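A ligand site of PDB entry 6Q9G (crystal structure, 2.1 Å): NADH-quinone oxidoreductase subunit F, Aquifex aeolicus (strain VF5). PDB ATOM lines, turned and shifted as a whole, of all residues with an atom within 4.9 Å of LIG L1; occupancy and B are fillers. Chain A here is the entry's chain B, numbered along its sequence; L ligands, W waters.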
ATOM      1  N   GLY A  67       1.710 -12.318  -2.785  1.00  0.00           N
ATOM      2  CA  GLY A  67       2.831 -13.263  -2.897  1.00  0.00           C
ATOM      3  C   GLY A  67       2.763 -14.066  -4.188  1.00  0.00           C
ATOM      4  O   GLY A  67       3.815 -14.624  -4.584  1.00  0.00           O
ATOM      5  N   GLY A  68       1.562 -14.167  -4.787  1.00  0.00           N
ATOM      6  CA  GLY A  68       1.362 -14.722  -6.140  1.00  0.00           C
ATOM      7  C   GLY A  68       0.153 -15.640  -6.265  1.00  0.00           C
ATOM      8  O   GLY A  68      -0.294 -15.813  -7.407  1.00  0.00           O
ATOM      9  N   ALA A  69      -0.370 -16.209  -5.176  1.00  0.00           N
ATOM     10  CA  ALA A  69      -1.491 -17.178  -5.240  1.00  0.00           C
ATOM     11  C   ALA A  69      -2.831 -16.434  -5.229  1.00  0.00           C
ATOM     12  O   ALA A  69      -3.812 -17.042  -5.666  1.00  0.00           O
ATOM     13  CB  ALA A  69      -1.421 -18.188  -4.117  1.00  0.00           C
ATOM     14  N   PHE A  71      -4.782 -15.454  -2.675  1.00  0.00           N
ATOM     15  CA  PHE A  71      -5.772 -15.908  -1.658  1.00  0.00           C
ATOM     16  C   PHE A  71      -6.318 -14.701  -0.890  1.00  0.00           C
ATOM     17  O   PHE A  71      -5.555 -13.811  -0.515  1.00  0.00           O
ATOM     18  CB  PHE A  71      -5.157 -16.948  -0.722  1.00  0.00           C
ATOM     19  CG  PHE A  71      -6.162 -17.649   0.154  1.00  0.00           C
ATOM     20  CD1 PHE A  71      -6.840 -18.759  -0.317  1.00  0.00           C
ATOM     21  CD2 PHE A  71      -6.454 -17.173   1.416  1.00  0.00           C
ATOM     22  CE1 PHE A  71      -7.776 -19.394   0.495  1.00  0.00           C
ATOM     23  CE2 PHE A  71      -7.377 -17.805   2.223  1.00  0.00           C
ATOM     24  CZ  PHE A  71      -8.036 -18.924   1.756  1.00  0.00           C
ATOM     25  N   LYS A  76      -8.119 -15.470   5.050  1.00  0.00           N
ATOM     26  CA  LYS A  76      -6.994 -16.213   5.684  1.00  0.00           C
ATOM     27  C   LYS A  76      -7.005 -15.914   7.183  1.00  0.00           C
ATOM     28  O   LYS A  76      -6.970 -16.862   7.977  1.00  0.00           O
ATOM     29  CB  LYS A  76      -5.647 -15.840   5.080  1.00  0.00           C
ATOM     30  CG  LYS A  76      -4.502 -16.751   5.480  1.00  0.00           C
ATOM     31  CD  LYS A  76      -3.149 -16.273   5.002  1.00  0.00           C
ATOM     32  CE  LYS A  76      -3.045 -16.246   3.481  1.00  0.00           C
ATOM     33  NZ  LYS A  76      -1.651 -16.034   3.056  1.00  0.00           N
ATOM     34  N   PHE A  79      -9.857 -17.614   9.229  1.00  0.00           N
ATOM     35  CA  PHE A  79      -9.510 -19.052   9.463  1.00  0.00           C
ATOM     36  C   PHE A  79      -8.588 -19.165  10.682  1.00  0.00           C
ATOM     37  O   PHE A  79      -8.838 -20.028  11.529  1.00  0.00           O
ATOM     38  CB  PHE A  79      -8.853 -19.699   8.242  1.00  0.00           C
ATOM     39  CG  PHE A  79      -9.799 -20.197   7.177  1.00  0.00           C
ATOM     40  CD1 PHE A  79     -10.736 -21.185   7.464  1.00  0.00           C
ATOM     41  CD2 PHE A  79      -9.741 -19.708   5.879  1.00  0.00           C
ATOM     42  CE1 PHE A  79     -11.592 -21.654   6.474  1.00  0.00           C
ATOM     43  CE2 PHE A  79     -10.600 -20.178   4.899  1.00  0.00           C
ATOM     44  CZ  PHE A  79     -11.519 -21.155   5.193  1.00  0.00           C
ATOM     45  N   GLU A  95      11.165 -13.510  -1.232  1.00  0.00           N
ATOM     46  CA  GLU A  95      11.111 -13.086  -2.660  1.00  0.00           C
ATOM     47  C   GLU A  95      12.299 -13.647  -3.450  1.00  0.00           C
ATOM     48  O   GLU A  95      13.370 -13.032  -3.429  1.00  0.00           O
ATOM     49  CB  GLU A  95      11.071 -11.549  -2.720  1.00  0.00           C
ATOM     50  CG  GLU A  95      11.089 -10.997  -4.136  1.00  0.00           C
ATOM     51  CD  GLU A  95      10.766  -9.517  -4.219  1.00  0.00           C
ATOM     52  OE1 GLU A  95      11.661  -8.681  -3.950  1.00  0.00           O
ATOM     53  OE2 GLU A  95       9.596  -9.194  -4.566  1.00  0.00           O
ATOM     54  N   SER A  96      12.099 -14.770  -4.136  1.00  0.00           N
ATOM     55  CA  SER A  96      13.161 -15.443  -4.940  1.00  0.00           C
ATOM     56  C   SER A  96      12.645 -15.917  -6.303  1.00  0.00           C
ATOM     57  O   SER A  96      13.433 -16.571  -7.009  1.00  0.00           O
ATOM     58  CB  SER A  96      13.778 -16.573  -4.158  1.00  0.00           C
ATOM     59  OG  SER A  96      14.404 -16.073  -2.979  1.00  0.00           O
ATOM     60  N   GLU A  97      11.404 -15.585  -6.692  1.00  0.00           N
ATOM     61  CA  GLU A  97      10.901 -15.852  -8.069  1.00  0.00           C
ATOM     62  C   GLU A  97      11.715 -15.023  -9.066  1.00  0.00           C
ATOM     63  O   GLU A  97      11.928 -13.832  -8.863  1.00  0.00           O
ATOM     64  CB  GLU A  97       9.417 -15.511  -8.192  1.00  0.00           C
ATOM     65  CG  GLU A  97       8.765 -15.987  -9.491  1.00  0.00           C
ATOM     66  CD  GLU A  97       8.481 -17.486  -9.578  1.00  0.00           C
ATOM     67  OE1 GLU A  97       8.988 -18.231  -8.721  1.00  0.00           O
ATOM     68  OE2 GLU A  97       7.734 -17.893 -10.492  1.00  0.00           O
ATOM     69  N   THR A 100      11.200 -10.948 -10.083  1.00  0.00           N
ATOM     70  CA  THR A 100      10.284 -10.490  -9.005  1.00  0.00           C
ATOM     71  C   THR A 100      11.083  -9.710  -7.959  1.00  0.00           C
ATOM     72  O   THR A 100      11.615 -10.351  -7.034  1.00  0.00           O
ATOM     73  CB  THR A 100       9.527 -11.668  -8.388  1.00  0.00           C
ATOM     74  OG1 THR A 100       8.995 -12.449  -9.447  1.00  0.00           O
ATOM     75  CG2 THR A 100       8.411 -11.207  -7.477  1.00  0.00           C
ATOM     76  N   ASP A 103       9.006  -6.681  -3.803  1.00  0.00           N
ATOM     77  CA  ASP A 103       8.971  -6.605  -2.317  1.00  0.00           C
ATOM     78  C   ASP A 103      10.202  -5.850  -1.800  1.00  0.00           C
ATOM     79  O   ASP A 103      10.077  -5.142  -0.775  1.00  0.00           O
ATOM     80  CB  ASP A 103       8.891  -7.985  -1.643  1.00  0.00           C
ATOM     81  CG  ASP A 103       7.667  -8.822  -2.002  1.00  0.00           C
ATOM     82  OD1 ASP A 103       6.679  -8.245  -2.505  1.00  0.00           O
ATOM     83  OD2 ASP A 103       7.701 -10.039  -1.753  1.00  0.00           O
ATOM     84  N   TYR A 180      15.269 -21.094  -2.493  1.00  0.00           N
ATOM     85  CA  TYR A 180      13.985 -20.645  -3.098  1.00  0.00           C
ATOM     86  C   TYR A 180      12.797 -21.275  -2.352  1.00  0.00           C
ATOM     87  O   TYR A 180      11.780 -20.590  -2.188  1.00  0.00           O
ATOM     88  CB  TYR A 180      13.969 -21.054  -4.561  1.00  0.00           C
ATOM     89  CG  TYR A 180      12.660 -20.925  -5.292  1.00  0.00           C
ATOM     90  CD1 TYR A 180      12.161 -19.692  -5.703  1.00  0.00           C
ATOM     91  CD2 TYR A 180      11.972 -22.056  -5.695  1.00  0.00           C
ATOM     92  CE1 TYR A 180      10.992 -19.599  -6.439  1.00  0.00           C
ATOM     93  CE2 TYR A 180      10.807 -21.981  -6.444  1.00  0.00           C
ATOM     94  CZ  TYR A 180      10.318 -20.742  -6.819  1.00  0.00           C
ATOM     95  OH  TYR A 180       9.175 -20.685  -7.564  1.00  0.00           O
ATOM     96  N   GLU A 185       5.421 -21.340   2.352  1.00  0.00           N
ATOM     97  CA  GLU A 185       5.071 -20.908   3.738  1.00  0.00           C
ATOM     98  C   GLU A 185       5.432 -22.005   4.755  1.00  0.00           C
ATOM     99  O   GLU A 185       5.939 -21.646   5.840  1.00  0.00           O
ATOM    100  CB  GLU A 185       3.597 -20.489   3.800  1.00  0.00           C
ATOM    101  CG  GLU A 185       2.632 -21.558   3.332  1.00  0.00           C
ATOM    102  CD  GLU A 185       1.180 -21.208   3.538  1.00  0.00           C
ATOM    103  OE1 GLU A 185       0.906 -20.030   3.918  1.00  0.00           O
ATOM    104  OE2 GLU A 185       0.331 -22.088   3.329  1.00  0.00           O
ATOM    105  N   TYR A 205      -3.213 -26.177   6.803  1.00  0.00           N
ATOM    106  CA  TYR A 205      -2.629 -24.866   6.410  1.00  0.00           C
ATOM    107  C   TYR A 205      -2.071 -24.222   7.677  1.00  0.00           C
ATOM    108  O   TYR A 205      -2.512 -24.501   8.787  1.00  0.00           O
ATOM    109  CB  TYR A 205      -3.636 -24.012   5.651  1.00  0.00           C
ATOM    110  CG  TYR A 205      -4.019 -24.599   4.321  1.00  0.00           C
ATOM    111  CD1 TYR A 205      -3.238 -24.412   3.183  1.00  0.00           C
ATOM    112  CD2 TYR A 205      -5.165 -25.369   4.198  1.00  0.00           C
ATOM    113  CE1 TYR A 205      -3.575 -24.979   1.966  1.00  0.00           C
ATOM    114  CE2 TYR A 205      -5.523 -25.938   2.985  1.00  0.00           C
ATOM    115  CZ  TYR A 205      -4.716 -25.752   1.866  1.00  0.00           C
ATOM    116  OH  TYR A 205      -5.083 -26.327   0.680  1.00  0.00           O
ATOM    117  N   PRO A 206      -1.058 -23.337   7.534  1.00  0.00           N
ATOM    118  CA  PRO A 206      -0.433 -22.702   8.692  1.00  0.00           C
ATOM    119  C   PRO A 206      -1.462 -22.090   9.667  1.00  0.00           C
ATOM    120  O   PRO A 206      -1.216 -22.126  10.849  1.00  0.00           O
ATOM    121  CB  PRO A 206       0.457 -21.649   8.043  1.00  0.00           C
ATOM    122  CG  PRO A 206       0.842 -22.258   6.712  1.00  0.00           C
ATOM    123  CD  PRO A 206      -0.437 -22.937   6.267  1.00  0.00           C
ATOM    124  N   VAL A 207      -2.575 -21.563   9.138  1.00  0.00           N
ATOM    125  CA  VAL A 207      -3.630 -20.869   9.948  1.00  0.00           C
ATOM    126  C   VAL A 207      -4.222 -21.852  10.967  1.00  0.00           C
ATOM    127  O   VAL A 207      -4.738 -21.389  12.010  1.00  0.00           O
ATOM    128  CB  VAL A 207      -4.718 -20.229   9.054  1.00  0.00           C
ATOM    129  CG1 VAL A 207      -4.182 -19.025   8.299  1.00  0.00           C
ATOM    130  CG2 VAL A 207      -5.338 -21.224   8.080  1.00  0.00           C
ATOM    131  N   VAL A 218       0.756 -16.525   7.380  1.00  0.00           N
ATOM    132  CA  VAL A 218       1.900 -16.127   6.518  1.00  0.00           C
ATOM    133  C   VAL A 218       1.334 -15.205   5.450  1.00  0.00           C
ATOM    134  O   VAL A 218       0.364 -15.618   4.774  1.00  0.00           O
ATOM    135  CB  VAL A 218       2.618 -17.323   5.868  1.00  0.00           C
ATOM    136  CG1 VAL A 218       3.760 -16.852   4.996  1.00  0.00           C
ATOM    137  CG2 VAL A 218       3.097 -18.302   6.921  1.00  0.00           C
ATOM    138  N   ASN A 220       2.630 -12.120   2.354  1.00  0.00           N
ATOM    139  CA  ASN A 220       3.683 -11.483   1.536  1.00  0.00           C
ATOM    140  C   ASN A 220       3.867 -10.023   1.977  1.00  0.00           C
ATOM    141  O   ASN A 220       2.854  -9.364   2.328  1.00  0.00           O
ATOM    142  CB  ASN A 220       3.345 -11.637   0.049  1.00  0.00           C
ATOM    143  CG  ASN A 220       4.247 -10.842  -0.853  1.00  0.00           C
ATOM    144  OD1 ASN A 220       3.864  -9.754  -1.306  1.00  0.00           O
ATOM    145  ND2 ASN A 220       5.453 -11.336  -1.085  1.00  0.00           N
ATOM    146  N   LEU A 297       6.595 -19.206 -13.810  1.00  0.00           N
ATOM    147  CA  LEU A 297       5.247 -19.822 -13.587  1.00  0.00           C
ATOM    148  C   LEU A 297       4.502 -19.989 -14.915  1.00  0.00           C
ATOM    149  O   LEU A 297       4.019 -21.119 -15.171  1.00  0.00           O
ATOM    150  CB  LEU A 297       4.451 -18.908 -12.639  1.00  0.00           C
ATOM    151  CG  LEU A 297       3.038 -19.382 -12.306  1.00  0.00           C
ATOM    152  CD1 LEU A 297       3.077 -20.742 -11.613  1.00  0.00           C
ATOM    153  CD2 LEU A 297       2.296 -18.359 -11.450  1.00  0.00           C
ATOM    154  N   GLY A 318      -0.484 -14.374 -10.846  1.00  0.00           N
ATOM    155  CA  GLY A 318       0.871 -14.594 -10.307  1.00  0.00           C
ATOM    156  C   GLY A 318       1.339 -13.411  -9.486  1.00  0.00           C
ATOM    157  O   GLY A 318       0.513 -12.786  -8.818  1.00  0.00           O
ATOM    158  N   THR A 319       2.640 -13.109  -9.533  1.00  0.00           N
ATOM    159  CA  THR A 319       3.287 -12.033  -8.759  1.00  0.00           C
ATOM    160  C   THR A 319       3.085 -10.688  -9.463  1.00  0.00           C
ATOM    161  O   THR A 319       3.375  -9.679  -8.842  1.00  0.00           O
ATOM    162  CB  THR A 319       4.778 -12.343  -8.565  1.00  0.00           C
ATOM    163  OG1 THR A 319       5.347 -12.522  -9.861  1.00  0.00           O
ATOM    164  CG2 THR A 319       5.042 -13.596  -7.742  1.00  0.00           C
ATOM    165  N   GLY A 394       3.792 -26.364  -4.226  1.00  0.00           N
ATOM    166  CA  GLY A 394       3.527 -25.735  -5.526  1.00  0.00           C
ATOM    167  C   GLY A 394       4.699 -25.828  -6.484  1.00  0.00           C
ATOM    168  O   GLY A 394       4.460 -25.657  -7.684  1.00  0.00           O
HETATM  169  P1  LIG L   1      -1.867 -21.719  -2.457  1.00  0.00           P
HETATM  170  O1  LIG L   1      -2.892 -21.235  -3.422  1.00  0.00           O
HETATM  171  O2  LIG L   1      -1.864 -23.180  -2.163  1.00  0.00           O
HETATM  172  O3  LIG L   1      -1.990 -20.956  -1.020  1.00  0.00           O
HETATM  173  C1  LIG L   1      -2.070 -19.504  -0.936  1.00  0.00           C
HETATM  174  C2  LIG L   1      -2.257 -19.051   0.493  1.00  0.00           C
HETATM  175  O4  LIG L   1      -3.623 -19.288   0.901  1.00  0.00           O
HETATM  176  C3  LIG L   1      -1.382 -19.734   1.537  1.00  0.00           C
HETATM  177  O5  LIG L   1      -1.066 -18.832   2.592  1.00  0.00           O
HETATM  178  C4  LIG L   1      -2.287 -20.877   2.018  1.00  0.00           C
HETATM  179  O6  LIG L   1      -2.007 -21.287   3.360  1.00  0.00           O
HETATM  180  C5  LIG L   1      -3.663 -20.219   1.961  1.00  0.00           C
HETATM  181  N1  LIG L   1      -4.757 -21.163   1.740  1.00  0.00           N
HETATM  182  C6  LIG L   1      -5.087 -21.819   0.584  1.00  0.00           C
HETATM  183  N2  LIG L   1      -6.114 -22.629   0.692  1.00  0.00           N
HETATM  184  C7  LIG L   1      -6.491 -22.495   2.019  1.00  0.00           C
HETATM  185  C8  LIG L   1      -7.498 -23.121   2.790  1.00  0.00           C
HETATM  186  N3  LIG L   1      -8.342 -24.044   2.311  1.00  0.00           N
HETATM  187  N4  LIG L   1      -7.593 -22.792   4.089  1.00  0.00           N
HETATM  188  C9  LIG L   1      -6.734 -21.890   4.591  1.00  0.00           C
HETATM  189  N5  LIG L   1      -5.744 -21.236   3.967  1.00  0.00           N
HETATM  190  C10 LIG L   1      -5.670 -21.599   2.678  1.00  0.00           C
HETATM  191  O7  LIG L   1      -0.414 -21.344  -2.996  1.00  0.00           O
HETATM  192  P2  LIG L   1       1.071 -21.537  -2.476  1.00  0.00           P
HETATM  193  O8  LIG L   1       1.494 -22.979  -2.812  1.00  0.00           O
HETATM  194  O9  LIG L   1       1.269 -21.113  -1.061  1.00  0.00           O
HETATM  195  O10 LIG L   1       1.838 -20.559  -3.484  1.00  0.00           O
HETATM  196  C11 LIG L   1       1.986 -20.670  -4.920  1.00  0.00           C
HETATM  197  C12 LIG L   1       2.366 -19.311  -5.442  1.00  0.00           C
HETATM  198  O11 LIG L   1       3.665 -18.933  -4.936  1.00  0.00           O
HETATM  199  C13 LIG L   1       2.476 -19.191  -6.967  1.00  0.00           C
HETATM  200  O12 LIG L   1       1.306 -18.615  -7.526  1.00  0.00           O
HETATM  201  C14 LIG L   1       3.690 -18.265  -7.189  1.00  0.00           C
HETATM  202  O13 LIG L   1       3.306 -17.093  -7.882  1.00  0.00           O
HETATM  203  C15 LIG L   1       4.099 -17.881  -5.769  1.00  0.00           C
HETATM  204  N6  LIG L   1       5.541 -17.689  -5.578  1.00  0.00           N
HETATM  205  C16 LIG L   1       6.078 -16.405  -5.291  1.00  0.00           C
HETATM  206  C17 LIG L   1       7.388 -16.172  -5.124  1.00  0.00           C
HETATM  207  C18 LIG L   1       7.845 -14.785  -4.833  1.00  0.00           C
HETATM  208  O14 LIG L   1       9.051 -14.524  -4.874  1.00  0.00           O
HETATM  209  N7  LIG L   1       6.941 -13.863  -4.542  1.00  0.00           N
HETATM  210  C19 LIG L   1       8.363 -17.304  -5.238  1.00  0.00           C
HETATM  211  C20 LIG L   1       7.697 -18.603  -5.515  1.00  0.00           C
HETATM  212  C21 LIG L   1       6.390 -18.745  -5.676  1.00  0.00           C
HETATM  213  N1  LG2 L   2       5.353 -16.164  -1.170  1.00  0.00           N
HETATM  214  C1  LG2 L   2       6.037 -15.032  -0.853  1.00  0.00           C
HETATM  215  O1  LG2 L   2       5.481 -14.064  -0.340  1.00  0.00           O
HETATM  216  N2  LG2 L   2       7.400 -14.977  -1.049  1.00  0.00           N
HETATM  217  C2  LG2 L   2       8.193 -15.995  -1.539  1.00  0.00           C
HETATM  218  O2  LG2 L   2       9.386 -15.806  -1.723  1.00  0.00           O
HETATM  219  C3  LG2 L   2       7.456 -17.227  -1.837  1.00  0.00           C
HETATM  220  N3  LG2 L   2       8.129 -18.269  -2.241  1.00  0.00           N
HETATM  221  C4  LG2 L   2       7.410 -19.427  -2.542  1.00  0.00           C
HETATM  222  C5  LG2 L   2       8.100 -20.549  -3.017  1.00  0.00           C
HETATM  223  C6  LG2 L   2       7.418 -21.703  -3.401  1.00  0.00           C
HETATM  224  C7  LG2 L   2       8.197 -22.891  -3.914  1.00  0.00           C
HETATM  225  C8  LG2 L   2       6.022 -21.748  -3.298  1.00  0.00           C
HETATM  226  C9  LG2 L   2       5.238 -22.949  -3.785  1.00  0.00           C
HETATM  227  C10 LG2 L   2       5.331 -20.652  -2.785  1.00  0.00           C
HETATM  228  C11 LG2 L   2       6.006 -19.488  -2.412  1.00  0.00           C
HETATM  229  N4  LG2 L   2       5.332 -18.335  -1.926  1.00  0.00           N
HETATM  230  C12 LG2 L   2       6.037 -17.196  -1.643  1.00  0.00           C
HETATM  231  C13 LG2 L   2       3.902 -18.340  -1.625  1.00  0.00           C
HETATM  232  C14 LG2 L   2       3.637 -18.681  -0.164  1.00  0.00           C
HETATM  233  O3  LG2 L   2       3.615 -20.106   0.002  1.00  0.00           O
HETATM  234  C15 LG2 L   2       2.330 -18.081   0.331  1.00  0.00           C
HETATM  235  O4  LG2 L   2       1.286 -18.354  -0.599  1.00  0.00           O
HETATM  236  C16 LG2 L   2       2.344 -16.570   0.570  1.00  0.00           C
HETATM  237  O5  LG2 L   2       3.585 -16.148   1.150  1.00  0.00           O
HETATM  238  C17 LG2 L   2       1.179 -16.151   1.448  1.00  0.00           C
HETATM  239  O6  LG2 L   2       1.055 -14.718   1.408  1.00  0.00           O
HETATM  240  P1  LG2 L   2      -0.017 -13.932   0.502  1.00  0.00           P
HETATM  241  O7  LG2 L   2       0.307 -13.938  -0.979  1.00  0.00           O
HETATM  242  O8  LG2 L   2      -1.376 -14.558   0.793  1.00  0.00           O
HETATM  243  O9  LG2 L   2      -0.012 -12.535   1.121  1.00  0.00           O
HETATM  244  O   HOH W   1      -9.130 -24.369   5.776  1.00  0.00           O
HETATM  245  O   HOH W   2      -4.365 -24.765  -1.802  1.00  0.00           O
HETATM  246  O   HOH W   3       1.003 -23.332   0.782  1.00  0.00           O
HETATM  247  O   HOH W   4       6.252 -21.494  -7.774  1.00  0.00           O
HETATM  248  O   HOH W   5      -0.792 -20.386  -7.507  1.00  0.00           O
HETATM  249  O   HOH W   6       7.404 -11.093  -4.195  1.00  0.00           O
HETATM  250  O   HOH W   7       5.203 -16.761  -9.616  1.00  0.00           O
HETATM  251  O   HOH W   8      -8.292 -25.355  -0.217  1.00  0.00           O
HETATM  252  O   HOH W   9       2.903 -24.981  -1.817  1.00  0.00           O
HETATM  253  O   HOH W  10      -6.765 -23.806  -1.637  1.00  0.00           O
HETATM  254  O   HOH W  11       0.454 -24.151  -5.175  1.00  0.00           O
HETATM  255  O   HOH W  12      -0.729 -18.612   5.955  1.00  0.00           O
HETATM  256  O   HOH W  13      -2.860 -20.439   5.626  1.00  0.00           O
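The side-chain carboxylate (OE2) of Glu 95 lies within hydrogen-bond range of the backbone NH (N) of Asp 103 (2.7 Å). The side-chain carboxylate of Glu 97 lies within hydrogen-bond range of the side-chain hydroxyl of Tyr 180 (2.7 Å). The side-chain hydroxyl of Thr 100 lies close to the backbone carbonyl oxygen of Glu 97, at 3.3 Å. The backbone carbonyl oxygen (O) of Val 218 lies within hydrogen-bond range of the side-chain amino group (NZ) of Lys 76.
Ala 69 touches LIG L1 (CB to O1, 3.5 Å). CG of Phe 71 touches O4 of LIG L1, 3.1 Å away. Phe 79 touches LIG L1 (CD2 to C9, 3.9 Å). Glu 95 touches LIG L1. OH of Tyr 180 touches C20 of LIG L1, 3.3 Å away. Tyr 205 touches LIG L1 (CD1 to O6, 3.4 Å). Pro 206 touches LIG L1. CG2 of Val 207 touches C9 of LIG L1 (3.8 Å). CD2 of Leu 297 touches O13 of LIG L1, at 3.9 Å. Thr 319 touches LIG L1. 16 residues have an atom within 4 Å of LIG L1: Gly 67, Gly 68, Ala 69, Phe 71, Lys 76, Phe 79, Glu 95, Ser 96, Glu 97, Tyr 180, Glu 185, Tyr 205, Pro 206, Val 207, Leu 297 and Thr 319.
O7 of LG2 L2 lies within hydrogen-bond range of N of Gly 67 (2.8 Å). The side-chain carboxylate (OE2) of Glu 185 lies within hydrogen-bond range of an oxygen (O6) of LIG L1, at 2.5 Å. The backbone NH (N) of Ser 96 sits at hydrogen-bond distance from an oxygen (O14) of LIG L1. O of Gly 67 sits close to N7 of LIG L1, at 3.2 Å. The side-chain amide nitrogen of Asn 220 lies within hydrogen-bond range of an oxygen (O1) of LG2 L2, 2.8 Å away. O2 of LG2 L2 sits at hydrogen-bond distance from N of Glu 95, 2.9 Å away. The backbone carbonyl oxygen (O) of Gly 68 sits at hydrogen-bond distance from an oxygen (O12) of LIG L1 (3.2 Å). The side-chain amino group (NZ) of Lys 76 is in salt-bridge range of an oxygen (O8) of LG2 L2 (2.7 Å). N of Glu 97 sits at hydrogen-bond distance from O14 of LIG L1 (3.2 Å). The side-chain amino group (NZ) of Lys 76 is in hydrogen-bond range of an oxygen (O5) of LIG L1, at 2.9 Å. N of Asn 220 lies within hydrogen-bond range of O9 of LG2 L2. The backbone NH (N) of Glu 185 is in hydrogen-bond range of an oxygen (O3) of LG2 L2, 3.2 Å away.
An oxygen (O3) of LG2 L2 lies within hydrogen-bond range of an oxygen (O9) of LIG L1.
Water W7 bridges O13 of LIG L1 (2.6 Å) and OE2 of Glu 97 (2.9 Å). Water W6 lies within hydrogen-bond range of the side-chain carboxylate of Asp 103 (2.7 Å), a nitrogen (N7) of LIG L1 (2.8 Å) and the side-chain carboxylate of Glu 95 (2.9 Å). Water W8 bridges a nitrogen (N3) of LIG L1 (2.8 Å) and the side-chain hydroxyl of Tyr 205 (3.5 Å). Water W3 bridges O9 of LIG L1 (2.9 Å) and OE2 of Glu 185 (2.9 Å). Water W2 lies within hydrogen-bond range of O2 of LIG L1 (3.0 Å) and OH of Tyr 205 (3.0 Å). Water W12 lies within hydrogen-bond range of N of Val 218 (2.9 Å), OE1 of Glu 185 (3.0 Å) and O5 of LIG L1 (3.4 Å).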
